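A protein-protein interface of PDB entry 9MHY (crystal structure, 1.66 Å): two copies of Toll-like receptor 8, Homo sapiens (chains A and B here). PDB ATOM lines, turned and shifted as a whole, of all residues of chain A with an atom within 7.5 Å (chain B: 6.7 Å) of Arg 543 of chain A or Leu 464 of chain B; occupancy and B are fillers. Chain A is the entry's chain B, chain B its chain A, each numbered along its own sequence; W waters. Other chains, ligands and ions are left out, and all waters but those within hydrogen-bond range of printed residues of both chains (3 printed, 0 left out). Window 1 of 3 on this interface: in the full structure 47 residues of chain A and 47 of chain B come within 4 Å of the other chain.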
ATOM      1  N   ARG A 515     -20.214  19.833  21.597  1.00  0.00           N
ATOM      2  CA  ARG A 515     -21.084  18.731  21.154  1.00  0.00           C
ATOM      3  C   ARG A 515     -20.609  18.323  19.734  1.00  0.00           C
ATOM      4  O   ARG A 515     -21.400  18.078  18.829  1.00  0.00           O
ATOM      5  CB  ARG A 515     -22.588  19.120  21.237  1.00  0.00           C
ATOM      6  CG  ARG A 515     -22.913  20.600  21.135  1.00  0.00           C
ATOM      7  CD  ARG A 515     -24.408  20.849  20.987  1.00  0.00           C
ATOM      8  NE  ARG A 515     -25.141  20.620  22.230  1.00  0.00           N
ATOM      9  CZ  ARG A 515     -26.473  20.593  22.332  1.00  0.00           C
ATOM     10  NH1 ARG A 515     -27.237  20.760  21.254  1.00  0.00           N
ATOM     11  NH2 ARG A 515     -27.050  20.393  23.511  1.00  0.00           N
ATOM     12  N   ASN A 538     -17.183  15.555  24.750  1.00  0.00           N
ATOM     13  CA  ASN A 538     -17.886  15.777  23.481  1.00  0.00           C
ATOM     14  C   ASN A 538     -18.732  14.512  23.217  1.00  0.00           C
ATOM     15  O   ASN A 538     -18.712  13.967  22.120  1.00  0.00           O
ATOM     16  CB  ASN A 538     -16.888  16.015  22.341  1.00  0.00           C
ATOM     17  CG  ASN A 538     -16.406  17.437  22.300  1.00  0.00           C
ATOM     18  OD1 ASN A 538     -17.147  18.321  21.898  1.00  0.00           O
ATOM     19  ND2 ASN A 538     -15.179  17.697  22.714  1.00  0.00           N
ATOM     20  N   SER A 539     -19.440  14.029  24.249  1.00  0.00           N
ATOM     21  CA  SER A 539     -20.200  12.786  24.161  1.00  0.00           C
ATOM     22  C   SER A 539     -21.475  12.868  23.350  1.00  0.00           C
ATOM     23  O   SER A 539     -22.036  11.814  23.033  1.00  0.00           O
ATOM     24  CB  SER A 539     -20.583  12.312  25.562  1.00  0.00           C
ATOM     25  OG  SER A 539     -21.489  13.221  26.163  1.00  0.00           O
ATOM     26  N   HIS A 540     -21.974  14.088  23.054  1.00  0.00           N
ATOM     27  CA  HIS A 540     -23.279  14.285  22.409  1.00  0.00           C
ATOM     28  C   HIS A 540     -23.630  13.282  21.298  1.00  0.00           C
ATOM     29  O   HIS A 540     -24.686  12.651  21.366  1.00  0.00           O
ATOM     30  CB  HIS A 540     -23.440  15.727  21.877  1.00  0.00           C
ATOM     31  CG  HIS A 540     -24.828  16.026  21.384  1.00  0.00           C
ATOM     32  ND1 HIS A 540     -25.662  16.887  22.069  1.00  0.00           N
ATOM     33  CD2 HIS A 540     -25.485  15.560  20.291  1.00  0.00           C
ATOM     34  CE1 HIS A 540     -26.795  16.923  21.383  1.00  0.00           C
ATOM     35  NE2 HIS A 540     -26.744  16.124  20.314  1.00  0.00           N
ATOM     36  N   TYR A 541     -22.784  13.175  20.265  1.00  0.00           N
ATOM     37  CA  TYR A 541     -23.075  12.301  19.135  1.00  0.00           C
ATOM     38  C   TYR A 541     -22.534  10.892  19.322  1.00  0.00           C
ATOM     39  O   TYR A 541     -23.149   9.946  18.816  1.00  0.00           O
ATOM     40  CB  TYR A 541     -22.579  12.931  17.820  1.00  0.00           C
ATOM     41  CG  TYR A 541     -23.470  14.073  17.383  1.00  0.00           C
ATOM     42  CD1 TYR A 541     -24.725  13.826  16.839  1.00  0.00           C
ATOM     43  CD2 TYR A 541     -23.141  15.387  17.681  1.00  0.00           C
ATOM     44  CE1 TYR A 541     -25.593  14.865  16.530  1.00  0.00           C
ATOM     45  CE2 TYR A 541     -23.977  16.438  17.328  1.00  0.00           C
ATOM     46  CZ  TYR A 541     -25.206  16.174  16.753  1.00  0.00           C
ATOM     47  OH  TYR A 541     -26.071  17.218  16.503  1.00  0.00           O
ATOM     48  N   PHE A 542     -21.427  10.721  20.080  1.00  0.00           N
ATOM     49  CA  PHE A 542     -20.915   9.368  20.352  1.00  0.00           C
ATOM     50  C   PHE A 542     -21.962   8.509  21.080  1.00  0.00           C
ATOM     51  O   PHE A 542     -21.975   7.292  20.893  1.00  0.00           O
ATOM     52  CB  PHE A 542     -19.652   9.409  21.224  1.00  0.00           C
ATOM     53  CG  PHE A 542     -18.380   9.815  20.519  1.00  0.00           C
ATOM     54  CD1 PHE A 542     -17.897   9.077  19.449  1.00  0.00           C
ATOM     55  CD2 PHE A 542     -17.655  10.914  20.941  1.00  0.00           C
ATOM     56  CE1 PHE A 542     -16.716   9.435  18.817  1.00  0.00           C
ATOM     57  CE2 PHE A 542     -16.461  11.258  20.316  1.00  0.00           C
ATOM     58  CZ  PHE A 542     -16.007  10.528  19.251  1.00  0.00           C
ATOM     59  N   ARG A 543     -22.802   9.126  21.928  1.00  0.00           N
ATOM     60  CA  ARG A 543     -23.778   8.352  22.692  1.00  0.00           C
ATOM     61  C   ARG A 543     -24.982   7.864  21.837  1.00  0.00           C
ATOM     62  O   ARG A 543     -25.687   6.973  22.287  1.00  0.00           O
ATOM     63  CB  ARG A 543     -24.224   9.093  23.957  1.00  0.00           C
ATOM     64  CG  ARG A 543     -25.125  10.266  23.741  1.00  0.00           C
ATOM     65  CD  ARG A 543     -25.076  11.165  24.966  1.00  0.00           C
ATOM     66  NE  ARG A 543     -25.948  12.329  24.798  1.00  0.00           N
ATOM     67  CZ  ARG A 543     -25.751  13.533  25.340  1.00  0.00           C
ATOM     68  NH1 ARG A 543     -24.687  13.763  26.114  1.00  0.00           N
ATOM     69  NH2 ARG A 543     -26.605  14.519  25.102  1.00  0.00           N
ATOM     70  N   ILE A 544     -25.152   8.359  20.592  1.00  0.00           N
ATOM     71  CA  ILE A 544     -26.236   7.949  19.695  1.00  0.00           C
ATOM     72  C   ILE A 544     -25.727   6.808  18.795  1.00  0.00           C
ATOM     73  O   ILE A 544     -24.867   7.048  17.949  1.00  0.00           O
ATOM     74  CB  ILE A 544     -26.712   9.154  18.815  1.00  0.00           C
ATOM     75  CG1 ILE A 544     -26.946  10.435  19.675  1.00  0.00           C
ATOM     76  CG2 ILE A 544     -27.990   8.749  18.017  1.00  0.00           C
ATOM     77  CD1 ILE A 544     -27.034  11.700  18.864  1.00  0.00           C
ATOM     78  N   ALA A 545     -26.267   5.592  18.950  1.00  0.00           N
ATOM     79  CA  ALA A 545     -25.806   4.462  18.135  1.00  0.00           C
ATOM     80  C   ALA A 545     -26.047   4.645  16.637  1.00  0.00           C
ATOM     81  O   ALA A 545     -25.198   4.263  15.830  1.00  0.00           O
ATOM     82  CB  ALA A 545     -26.462   3.162  18.604  1.00  0.00           C
ATOM     83  N   GLY A 546     -27.211   5.189  16.288  1.00  0.00           N
ATOM     84  CA  GLY A 546     -27.671   5.311  14.911  1.00  0.00           C
ATOM     85  C   GLY A 546     -26.973   6.314  14.024  1.00  0.00           C
ATOM     86  O   GLY A 546     -27.197   6.288  12.812  1.00  0.00           O
ATOM     87  N   VAL A 547     -26.187   7.236  14.604  1.00  0.00           N
ATOM     88  CA  VAL A 547     -25.426   8.183  13.804  1.00  0.00           C
ATOM     89  C   VAL A 547     -24.020   7.623  13.585  1.00  0.00           C
ATOM     90  O   VAL A 547     -23.584   6.738  14.322  1.00  0.00           O
ATOM     91  CB  VAL A 547     -25.407   9.613  14.383  1.00  0.00           C
ATOM     92  CG1 VAL A 547     -26.817  10.076  14.715  1.00  0.00           C
ATOM     93  CG2 VAL A 547     -24.491   9.715  15.603  1.00  0.00           C
ATOM     94  N   HIS A 549     -19.836   7.627  13.383  1.00  0.00           N
ATOM     95  CA  HIS A 549     -18.758   8.196  14.207  1.00  0.00           C
ATOM     96  C   HIS A 549     -17.436   7.818  13.552  1.00  0.00           C
ATOM     97  O   HIS A 549     -17.207   6.651  13.272  1.00  0.00           O
ATOM     98  CB  HIS A 549     -18.791   7.657  15.653  1.00  0.00           C
ATOM     99  CG  HIS A 549     -20.158   7.565  16.261  1.00  0.00           C
ATOM    100  ND1 HIS A 549     -20.918   6.419  16.151  1.00  0.00           N
ATOM    101  CD2 HIS A 549     -20.863   8.491  16.944  1.00  0.00           C
ATOM    102  CE1 HIS A 549     -22.046   6.675  16.782  1.00  0.00           C
ATOM    103  NE2 HIS A 549     -22.067   7.922  17.246  1.00  0.00           N
ATOM    104  N   ASN A 568     -16.297  10.790  26.686  1.00  0.00           N
ATOM    105  CA  ASN A 568     -16.976  10.870  25.402  1.00  0.00           C
ATOM    106  C   ASN A 568     -18.023   9.771  25.226  1.00  0.00           C
ATOM    107  O   ASN A 568     -18.745   9.805  24.234  1.00  0.00           O
ATOM    108  CB  ASN A 568     -15.961  10.839  24.267  1.00  0.00           C
ATOM    109  CG  ASN A 568     -15.426  12.203  23.973  1.00  0.00           C
ATOM    110  OD1 ASN A 568     -16.215  13.120  23.868  1.00  0.00           O
ATOM    111  ND2 ASN A 568     -14.131  12.385  23.816  1.00  0.00           N
ATOM    112  N   ASN A 569     -18.139   8.806  26.178  1.00  0.00           N
ATOM    113  CA  ASN A 569     -19.131   7.735  26.087  1.00  0.00           C
ATOM    114  C   ASN A 569     -18.976   6.956  24.766  1.00  0.00           C
ATOM    115  O   ASN A 569     -19.967   6.558  24.165  1.00  0.00           O
ATOM    116  CB  ASN A 569     -20.552   8.351  26.224  1.00  0.00           C
ATOM    117  CG  ASN A 569     -21.322   7.906  27.434  1.00  0.00           C
ATOM    118  OD1 ASN A 569     -20.817   7.964  28.571  1.00  0.00           O
ATOM    119  ND2 ASN A 569     -22.549   7.437  27.237  1.00  0.00           N
ATOM    120  N   ILE A 570     -17.720   6.764  24.306  1.00  0.00           N
ATOM    121  CA  ILE A 570     -17.444   6.068  23.050  1.00  0.00           C
ATOM    122  C   ILE A 570     -17.746   4.586  23.214  1.00  0.00           C
ATOM    123  O   ILE A 570     -17.163   3.936  24.082  1.00  0.00           O
ATOM    124  CB  ILE A 570     -15.962   6.275  22.599  1.00  0.00           C
ATOM    125  CG1 ILE A 570     -15.669   7.791  22.359  1.00  0.00           C
ATOM    126  CG2 ILE A 570     -15.657   5.424  21.338  1.00  0.00           C
ATOM    127  CD1 ILE A 570     -14.180   8.193  22.181  1.00  0.00           C
ATOM    128  N   TYR A 571     -18.691   4.065  22.423  1.00  0.00           N
ATOM    129  CA  TYR A 571     -19.035   2.642  22.433  1.00  0.00           C
ATOM    130  C   TYR A 571     -19.230   2.050  21.054  1.00  0.00           C
ATOM    131  O   TYR A 571     -19.446   0.855  20.964  1.00  0.00           O
ATOM    132  CB  TYR A 571     -20.294   2.367  23.264  1.00  0.00           C
ATOM    133  CG  TYR A 571     -21.599   2.828  22.664  1.00  0.00           C
ATOM    134  CD1 TYR A 571     -21.980   4.158  22.742  1.00  0.00           C
ATOM    135  CD2 TYR A 571     -22.546   1.909  22.220  1.00  0.00           C
ATOM    136  CE1 TYR A 571     -23.238   4.573  22.342  1.00  0.00           C
ATOM    137  CE2 TYR A 571     -23.813   2.316  21.812  1.00  0.00           C
ATOM    138  CZ  TYR A 571     -24.158   3.651  21.892  1.00  0.00           C
ATOM    139  OH  TYR A 571     -25.411   4.091  21.561  1.00  0.00           O
ATOM    140  N   THR A 572     -19.196   2.863  19.976  1.00  0.00           N
ATOM    141  CA  THR A 572     -19.391   2.358  18.622  1.00  0.00           C
ATOM    142  C   THR A 572     -18.745   3.318  17.632  1.00  0.00           C
ATOM    143  O   THR A 572     -18.865   4.543  17.786  1.00  0.00           O
ATOM    144  CB  THR A 572     -20.900   2.148  18.323  1.00  0.00           C
ATOM    145  OG1 THR A 572     -21.042   1.660  16.988  1.00  0.00           O
ATOM    146  CG2 THR A 572     -21.735   3.419  18.507  1.00  0.00           C
ATOM    147  N   TYR B 398     -42.715  14.603  18.803  1.00  0.00           N
ATOM    148  CA  TYR B 398     -41.366  14.318  19.250  1.00  0.00           C
ATOM    149  C   TYR B 398     -40.335  14.673  18.175  1.00  0.00           C
ATOM    150  O   TYR B 398     -40.277  14.030  17.126  1.00  0.00           O
ATOM    151  CB  TYR B 398     -41.286  12.866  19.725  1.00  0.00           C
ATOM    152  CG  TYR B 398     -39.979  12.490  20.376  1.00  0.00           C
ATOM    153  CD1 TYR B 398     -39.787  12.652  21.744  1.00  0.00           C
ATOM    154  CD2 TYR B 398     -38.965  11.888  19.646  1.00  0.00           C
ATOM    155  CE1 TYR B 398     -38.600  12.263  22.353  1.00  0.00           C
ATOM    156  CE2 TYR B 398     -37.780  11.494  20.246  1.00  0.00           C
ATOM    157  CZ  TYR B 398     -37.621  11.636  21.609  1.00  0.00           C
ATOM    158  OH  TYR B 398     -36.432  11.279  22.205  1.00  0.00           O
ATOM    159  N   LEU B 399     -39.551  15.746  18.430  1.00  0.00           N
ATOM    160  CA  LEU B 399     -38.539  16.251  17.493  1.00  0.00           C
ATOM    161  C   LEU B 399     -37.140  16.304  18.145  1.00  0.00           C
ATOM    162  O   LEU B 399     -36.281  17.066  17.677  1.00  0.00           O
ATOM    163  CB  LEU B 399     -38.949  17.670  17.041  1.00  0.00           C
ATOM    164  CG  LEU B 399     -40.356  17.807  16.460  1.00  0.00           C
ATOM    165  CD1 LEU B 399     -40.740  19.273  16.284  1.00  0.00           C
ATOM    166  CD2 LEU B 399     -40.487  17.018  15.166  1.00  0.00           C
ATOM    167  N   SER B 400     -36.904  15.499  19.190  1.00  0.00           N
ATOM    168  CA  SER B 400     -35.645  15.499  19.920  1.00  0.00           C
ATOM    169  C   SER B 400     -34.505  15.060  19.013  1.00  0.00           C
ATOM    170  O   SER B 400     -34.701  14.203  18.150  1.00  0.00           O
ATOM    171  CB  SER B 400     -35.721  14.545  21.111  1.00  0.00           C
ATOM    172  OG  SER B 400     -34.523  14.477  21.869  1.00  0.00           O
ATOM    173  N   GLU B 401     -33.334  15.661  19.203  1.00  0.00           N
ATOM    174  CA  GLU B 401     -32.118  15.276  18.496  1.00  0.00           C
ATOM    175  C   GLU B 401     -32.172  15.550  17.004  1.00  0.00           C
ATOM    176  O   GLU B 401     -32.116  14.641  16.177  1.00  0.00           O
ATOM    177  CB  GLU B 401     -31.782  13.804  18.793  1.00  0.00           C
ATOM    178  CG  GLU B 401     -30.342  13.429  18.491  1.00  0.00           C
ATOM    179  CD  GLU B 401     -29.352  14.194  19.350  1.00  0.00           C
ATOM    180  OE1 GLU B 401     -28.757  15.177  18.857  1.00  0.00           O
ATOM    181  OE2 GLU B 401     -29.178  13.812  20.527  1.00  0.00           O
ATOM    182  N   ASN B 402     -32.268  16.814  16.664  1.00  0.00           N
ATOM    183  CA  ASN B 402     -32.250  17.268  15.276  1.00  0.00           C
ATOM    184  C   ASN B 402     -31.277  18.481  15.233  1.00  0.00           C
ATOM    185  O   ASN B 402     -30.393  18.562  16.100  1.00  0.00           O
ATOM    186  CB  ASN B 402     -33.722  17.552  14.821  1.00  0.00           C
ATOM    187  CG  ASN B 402     -34.405  16.285  14.348  1.00  0.00           C
ATOM    188  OD1 ASN B 402     -33.980  15.686  13.353  1.00  0.00           O
ATOM    189  ND2 ASN B 402     -35.425  15.836  15.061  1.00  0.00           N
ATOM    190  N   ARG B 403     -31.383  19.363  14.233  1.00  0.00           N
ATOM    191  CA  ARG B 403     -30.551  20.567  14.097  1.00  0.00           C
ATOM    192  C   ARG B 403     -31.454  21.806  14.018  1.00  0.00           C
ATOM    193  O   ARG B 403     -31.159  22.738  13.273  1.00  0.00           O
ATOM    194  CB  ARG B 403     -29.703  20.469  12.814  1.00  0.00           C
ATOM    195  CG  ARG B 403     -28.880  19.220  12.711  1.00  0.00           C
ATOM    196  CD  ARG B 403     -27.700  19.194  13.655  1.00  0.00           C
ATOM    197  NE  ARG B 403     -26.684  20.191  13.302  1.00  0.00           N
ATOM    198  CZ  ARG B 403     -25.471  20.247  13.838  1.00  0.00           C
ATOM    199  NH1 ARG B 403     -24.610  21.183  13.449  1.00  0.00           N
ATOM    200  NH2 ARG B 403     -25.095  19.353  14.749  1.00  0.00           N
ATOM    201  N   ILE B 404     -32.578  21.805  14.758  1.00  0.00           N
ATOM    202  CA  ILE B 404     -33.522  22.905  14.696  1.00  0.00           C
ATOM    203  C   ILE B 404     -32.868  24.106  15.369  1.00  0.00           C
ATOM    204  O   ILE B 404     -32.306  23.987  16.456  1.00  0.00           O
ATOM    205  CB  ILE B 404     -34.881  22.509  15.306  1.00  0.00           C
ATOM    206  CG1 ILE B 404     -35.526  21.367  14.461  1.00  0.00           C
ATOM    207  CG2 ILE B 404     -35.805  23.730  15.372  1.00  0.00           C
ATOM    208  CD1 ILE B 404     -36.576  20.521  15.241  1.00  0.00           C
ATOM    209  N   PHE B 444     -35.716   1.783  21.833  1.00  0.00           N
ATOM    210  CA  PHE B 444     -35.989   1.871  23.268  1.00  0.00           C
ATOM    211  C   PHE B 444     -37.507   1.789  23.466  1.00  0.00           C
ATOM    212  O   PHE B 444     -38.257   2.249  22.610  1.00  0.00           O
ATOM    213  CB  PHE B 444     -35.482   3.210  23.847  1.00  0.00           C
ATOM    214  CG  PHE B 444     -34.013   3.498  23.665  1.00  0.00           C
ATOM    215  CD1 PHE B 444     -33.057   2.573  24.048  1.00  0.00           C
ATOM    216  CD2 PHE B 444     -33.585   4.723  23.178  1.00  0.00           C
ATOM    217  CE1 PHE B 444     -31.699   2.863  23.930  1.00  0.00           C
ATOM    218  CE2 PHE B 444     -32.225   5.009  23.062  1.00  0.00           C
ATOM    219  CZ  PHE B 444     -31.295   4.078  23.437  1.00  0.00           C
ATOM    220  N   ASP B 461     -41.650  18.061  22.111  1.00  0.00           N
ATOM    221  CA  ASP B 461     -40.303  17.794  22.585  1.00  0.00           C
ATOM    222  C   ASP B 461     -39.287  18.292  21.556  1.00  0.00           C
ATOM    223  O   ASP B 461     -39.148  17.707  20.495  1.00  0.00           O
ATOM    224  CB  ASP B 461     -40.123  16.296  22.886  1.00  0.00           C
ATOM    225  CG  ASP B 461     -38.823  15.948  23.585  1.00  0.00           C
ATOM    226  OD1 ASP B 461     -37.846  16.705  23.440  1.00  0.00           O
ATOM    227  OD2 ASP B 461     -38.786  14.919  24.281  1.00  0.00           O
ATOM    228  N   LEU B 462     -38.600  19.388  21.881  1.00  0.00           N
ATOM    229  CA  LEU B 462     -37.554  19.975  21.043  1.00  0.00           C
ATOM    230  C   LEU B 462     -36.184  19.869  21.735  1.00  0.00           C
ATOM    231  O   LEU B 462     -35.284  20.681  21.460  1.00  0.00           O
ATOM    232  CB  LEU B 462     -37.901  21.457  20.767  1.00  0.00           C
ATOM    233  CG  LEU B 462     -39.006  21.702  19.742  1.00  0.00           C
ATOM    234  CD1 LEU B 462     -39.602  23.092  19.920  1.00  0.00           C
ATOM    235  CD2 LEU B 462     -38.487  21.510  18.307  1.00  0.00           C
ATOM    236  N   SER B 463     -36.005  18.865  22.620  1.00  0.00           N
ATOM    237  CA  SER B 463     -34.754  18.702  23.324  1.00  0.00           C
ATOM    238  C   SER B 463     -33.646  18.301  22.374  1.00  0.00           C
ATOM    239  O   SER B 463     -33.906  17.752  21.301  1.00  0.00           O
ATOM    240  CB  SER B 463     -34.887  17.653  24.419  1.00  0.00           C
ATOM    241  OG  SER B 463     -35.184  16.374  23.882  1.00  0.00           O
ATOM    242  N   LEU B 464     -32.395  18.605  22.758  1.00  0.00           N
ATOM    243  CA  LEU B 464     -31.239  18.231  21.961  1.00  0.00           C
ATOM    244  C   LEU B 464     -31.294  18.780  20.541  1.00  0.00           C
ATOM    245  O   LEU B 464     -31.084  18.058  19.569  1.00  0.00           O
ATOM    246  CB  LEU B 464     -31.032  16.706  21.991  1.00  0.00           C
ATOM    247  CG  LEU B 464     -30.772  16.117  23.403  1.00  0.00           C
ATOM    248  CD1 LEU B 464     -31.199  14.662  23.475  1.00  0.00           C
ATOM    249  CD2 LEU B 464     -29.309  16.264  23.788  1.00  0.00           C
ATOM    250  N   ASN B 465     -31.589  20.068  20.433  1.00  0.00           N
ATOM    251  CA  ASN B 465     -31.562  20.779  19.158  1.00  0.00           C
ATOM    252  C   ASN B 465     -30.594  21.980  19.369  1.00  0.00           C
ATOM    253  O   ASN B 465     -29.734  21.917  20.264  1.00  0.00           O
ATOM    254  CB  ASN B 465     -33.010  21.159  18.739  1.00  0.00           C
ATOM    255  CG  ASN B 465     -33.721  20.028  18.041  1.00  0.00           C
ATOM    256  OD1 ASN B 465     -33.465  19.785  16.862  1.00  0.00           O
ATOM    257  ND2 ASN B 465     -34.598  19.301  18.724  1.00  0.00           N
ATOM    258  N   SER B 466     -30.675  23.024  18.547  1.00  0.00           N
ATOM    259  CA  SER B 466     -29.821  24.201  18.631  1.00  0.00           C
ATOM    260  C   SER B 466     -30.681  25.472  18.676  1.00  0.00           C
ATOM    261  O   SER B 466     -30.371  26.450  17.997  1.00  0.00           O
ATOM    262  CB  SER B 466     -28.901  24.232  17.414  1.00  0.00           C
ATOM    263  OG  SER B 466     -28.152  23.036  17.346  1.00  0.00           O
ATOM    264  N   ASN B 485     -40.543  20.600  26.113  1.00  0.00           N
ATOM    265  CA  ASN B 485     -39.194  20.237  26.476  1.00  0.00           C
ATOM    266  C   ASN B 485     -38.190  20.954  25.567  1.00  0.00           C
ATOM    267  O   ASN B 485     -38.173  20.734  24.366  1.00  0.00           O
ATOM    268  CB  ASN B 485     -39.020  18.712  26.477  1.00  0.00           C
ATOM    269  CG  ASN B 485     -37.733  18.229  26.987  1.00  0.00           C
ATOM    270  OD1 ASN B 485     -36.894  19.018  27.456  1.00  0.00           O
ATOM    271  ND2 ASN B 485     -37.553  16.930  27.098  1.00  0.00           N
ATOM    272  N   LEU B 486     -37.410  21.870  26.151  1.00  0.00           N
ATOM    273  CA  LEU B 486     -36.341  22.600  25.469  1.00  0.00           C
ATOM    274  C   LEU B 486     -34.976  22.254  26.114  1.00  0.00           C
ATOM    275  O   LEU B 486     -34.029  23.045  26.041  1.00  0.00           O
ATOM    276  CB  LEU B 486     -36.614  24.108  25.562  1.00  0.00           C
ATOM    277  CG  LEU B 486     -37.788  24.623  24.727  1.00  0.00           C
ATOM    278  CD1 LEU B 486     -38.208  25.995  25.198  1.00  0.00           C
ATOM    279  CD2 LEU B 486     -37.420  24.692  23.225  1.00  0.00           C
ATOM    280  N   SER B 487     -34.860  21.066  26.727  1.00  0.00           N
ATOM    281  CA  SER B 487     -33.622  20.637  27.360  1.00  0.00           C
ATOM    282  C   SER B 487     -32.496  20.568  26.341  1.00  0.00           C
ATOM    283  O   SER B 487     -32.744  20.198  25.202  1.00  0.00           O
ATOM    284  CB  SER B 487     -33.798  19.251  27.974  1.00  0.00           C
ATOM    285  OG  SER B 487     -32.603  18.763  28.557  1.00  0.00           O
ATOM    286  N   ALA B 488     -31.259  20.894  26.759  1.00  0.00           N
ATOM    287  CA  ALA B 488     -30.063  20.743  25.918  1.00  0.00           C
ATOM    288  C   ALA B 488     -30.165  21.396  24.541  1.00  0.00           C
ATOM    289  O   ALA B 488     -29.986  20.748  23.514  1.00  0.00           O
ATOM    290  CB  ALA B 488     -29.688  19.258  25.791  1.00  0.00           C
ATOM    291  N   ASN B 489     -30.475  22.677  24.528  1.00  0.00           N
ATOM    292  CA  ASN B 489     -30.511  23.495  23.315  1.00  0.00           C
ATOM    293  C   ASN B 489     -29.431  24.578  23.328  1.00  0.00           C
ATOM    294  O   ASN B 489     -29.497  25.488  22.504  1.00  0.00           O
ATOM    295  CB  ASN B 489     -31.904  24.128  23.145  1.00  0.00           C
ATOM    296  CG  ASN B 489     -32.838  23.221  22.374  1.00  0.00           C
ATOM    297  OD1 ASN B 489     -32.823  23.209  21.144  1.00  0.00           O
ATOM    298  ND2 ASN B 489     -33.592  22.393  23.066  1.00  0.00           N
HETATM  299  O   HOH W   1     -28.676  16.339  16.333  1.00  0.00           O
HETATM  300  O   HOH W   2     -27.252  13.323  22.332  1.00  0.00           O
HETATM  301  O   HOH W   3     -28.193  18.753  18.995  1.00  0.00           O
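Printed residues of chain B within 4 Å of Arg 515 of chain A: Asn 465 (2.9 Å) and Ala 488 (3.0 Å).
Of the printed residues of chain B, Tyr 541 of chain A touches Glu 401 (3.9 Å) and Arg 403 (2.9 Å).
Arg 543 of chain A touches one residue of chain B.
Leu 462 of chain B touches none of the printed residues of chain A.
Of chain A, only His 540 (3.5 Å) and Arg 543 (3.5 Å) come within 4 Å of Leu 464 of chain B.
Printed residues of chain A within 4 Å of Asn 465 of chain B: Arg 515 (2.9 Å).
Of the printed residues of chain A, Ala 488 of chain B touches Arg 515.
Asn 489 of chain B touches none of the printed residues of chain A.
A ring nitrogen (NE2) of His 540 of chain A sits at hydrogen-bond distance from the side-chain carboxylate (OE1) of Glu 401 of chain B, at 2.7 Å.
NH2 of Arg 403 of chain B sits at hydrogen-bond distance from OH of Tyr 541 of chain A (2.9 Å).
O of Asn 465 of chain B sits at hydrogen-bond distance from NH1 of Arg 515 of chain A (2.9 Å).
The backbone carbonyl oxygen of Ala 488 of chain B is in hydrogen-bond range of the guanidinium group of Arg 515 of chain A (3.0 Å).
Among the printed residues, merely in contact across the chains: His 540 of chain A with Leu 464 of chain B, Tyr 541 of chain A with Glu 401 of chain B, Arg 543 of chain A with Leu 464 of chain B and Ile 544 of chain A with Glu 401 of chain B.
O of Leu 399 of chain B is in hydrogen-bond range of ND2 of Asn 465 of chain B, at 3.0 Å.
O of Ser 463 of chain B is in hydrogen-bond range of N of Glu 401 of chain B.
The side-chain amide oxygen (OD1) of Asn 465 of chain B sits close to the backbone NH (N) of Asn 402 of chain B (3.2 Å).
N of Asn 465 of chain B lies close to OD1 of Asn 489 of chain B (3.4 Å).
O of Tyr 541 of chain A sits at hydrogen-bond distance from NE2 of His 549 of chain A (2.8 Å).
The backbone carbonyl oxygen (O) of Ile 544 of chain A is in hydrogen-bond range of a ring nitrogen (NE2) of His 549 of chain A (3.0 Å).
No position is printed for both chains.
Of the 8 pairs that touch across the chains among the printed residues, none has its exchanged pair printed and touching as well.
Among the printed residues, 8 pairs touch across the chains.
Among the printed residues, no Asp or Glu carboxylate lies within 4 Å of a Lys or Arg side-chain nitrogen of the other chain.
Water W2 lies within hydrogen-bond range of OE2 of Glu 401 of chain B (2.7 Å), O of His 540 of chain A (2.8 Å) and NE of Arg 543 of chain A (3.0 Å).
Water W1 lies within hydrogen-bond range of the side-chain hydroxyl (OH) of Tyr 541 of chain A (2.8 Å), the side-chain carboxylate (OE1) of Glu 401 of chain B (2.8 Å) and the backbone carbonyl oxygen (O) of Asn 402 of chain B (2.8 Å).
Water W3 lies within hydrogen-bond range of O of Leu 464 of chain B (3.0 Å), NH1 of Arg 515 of chain A (3.2 Å) and NE2 of His 540 of chain A (3.3 Å).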
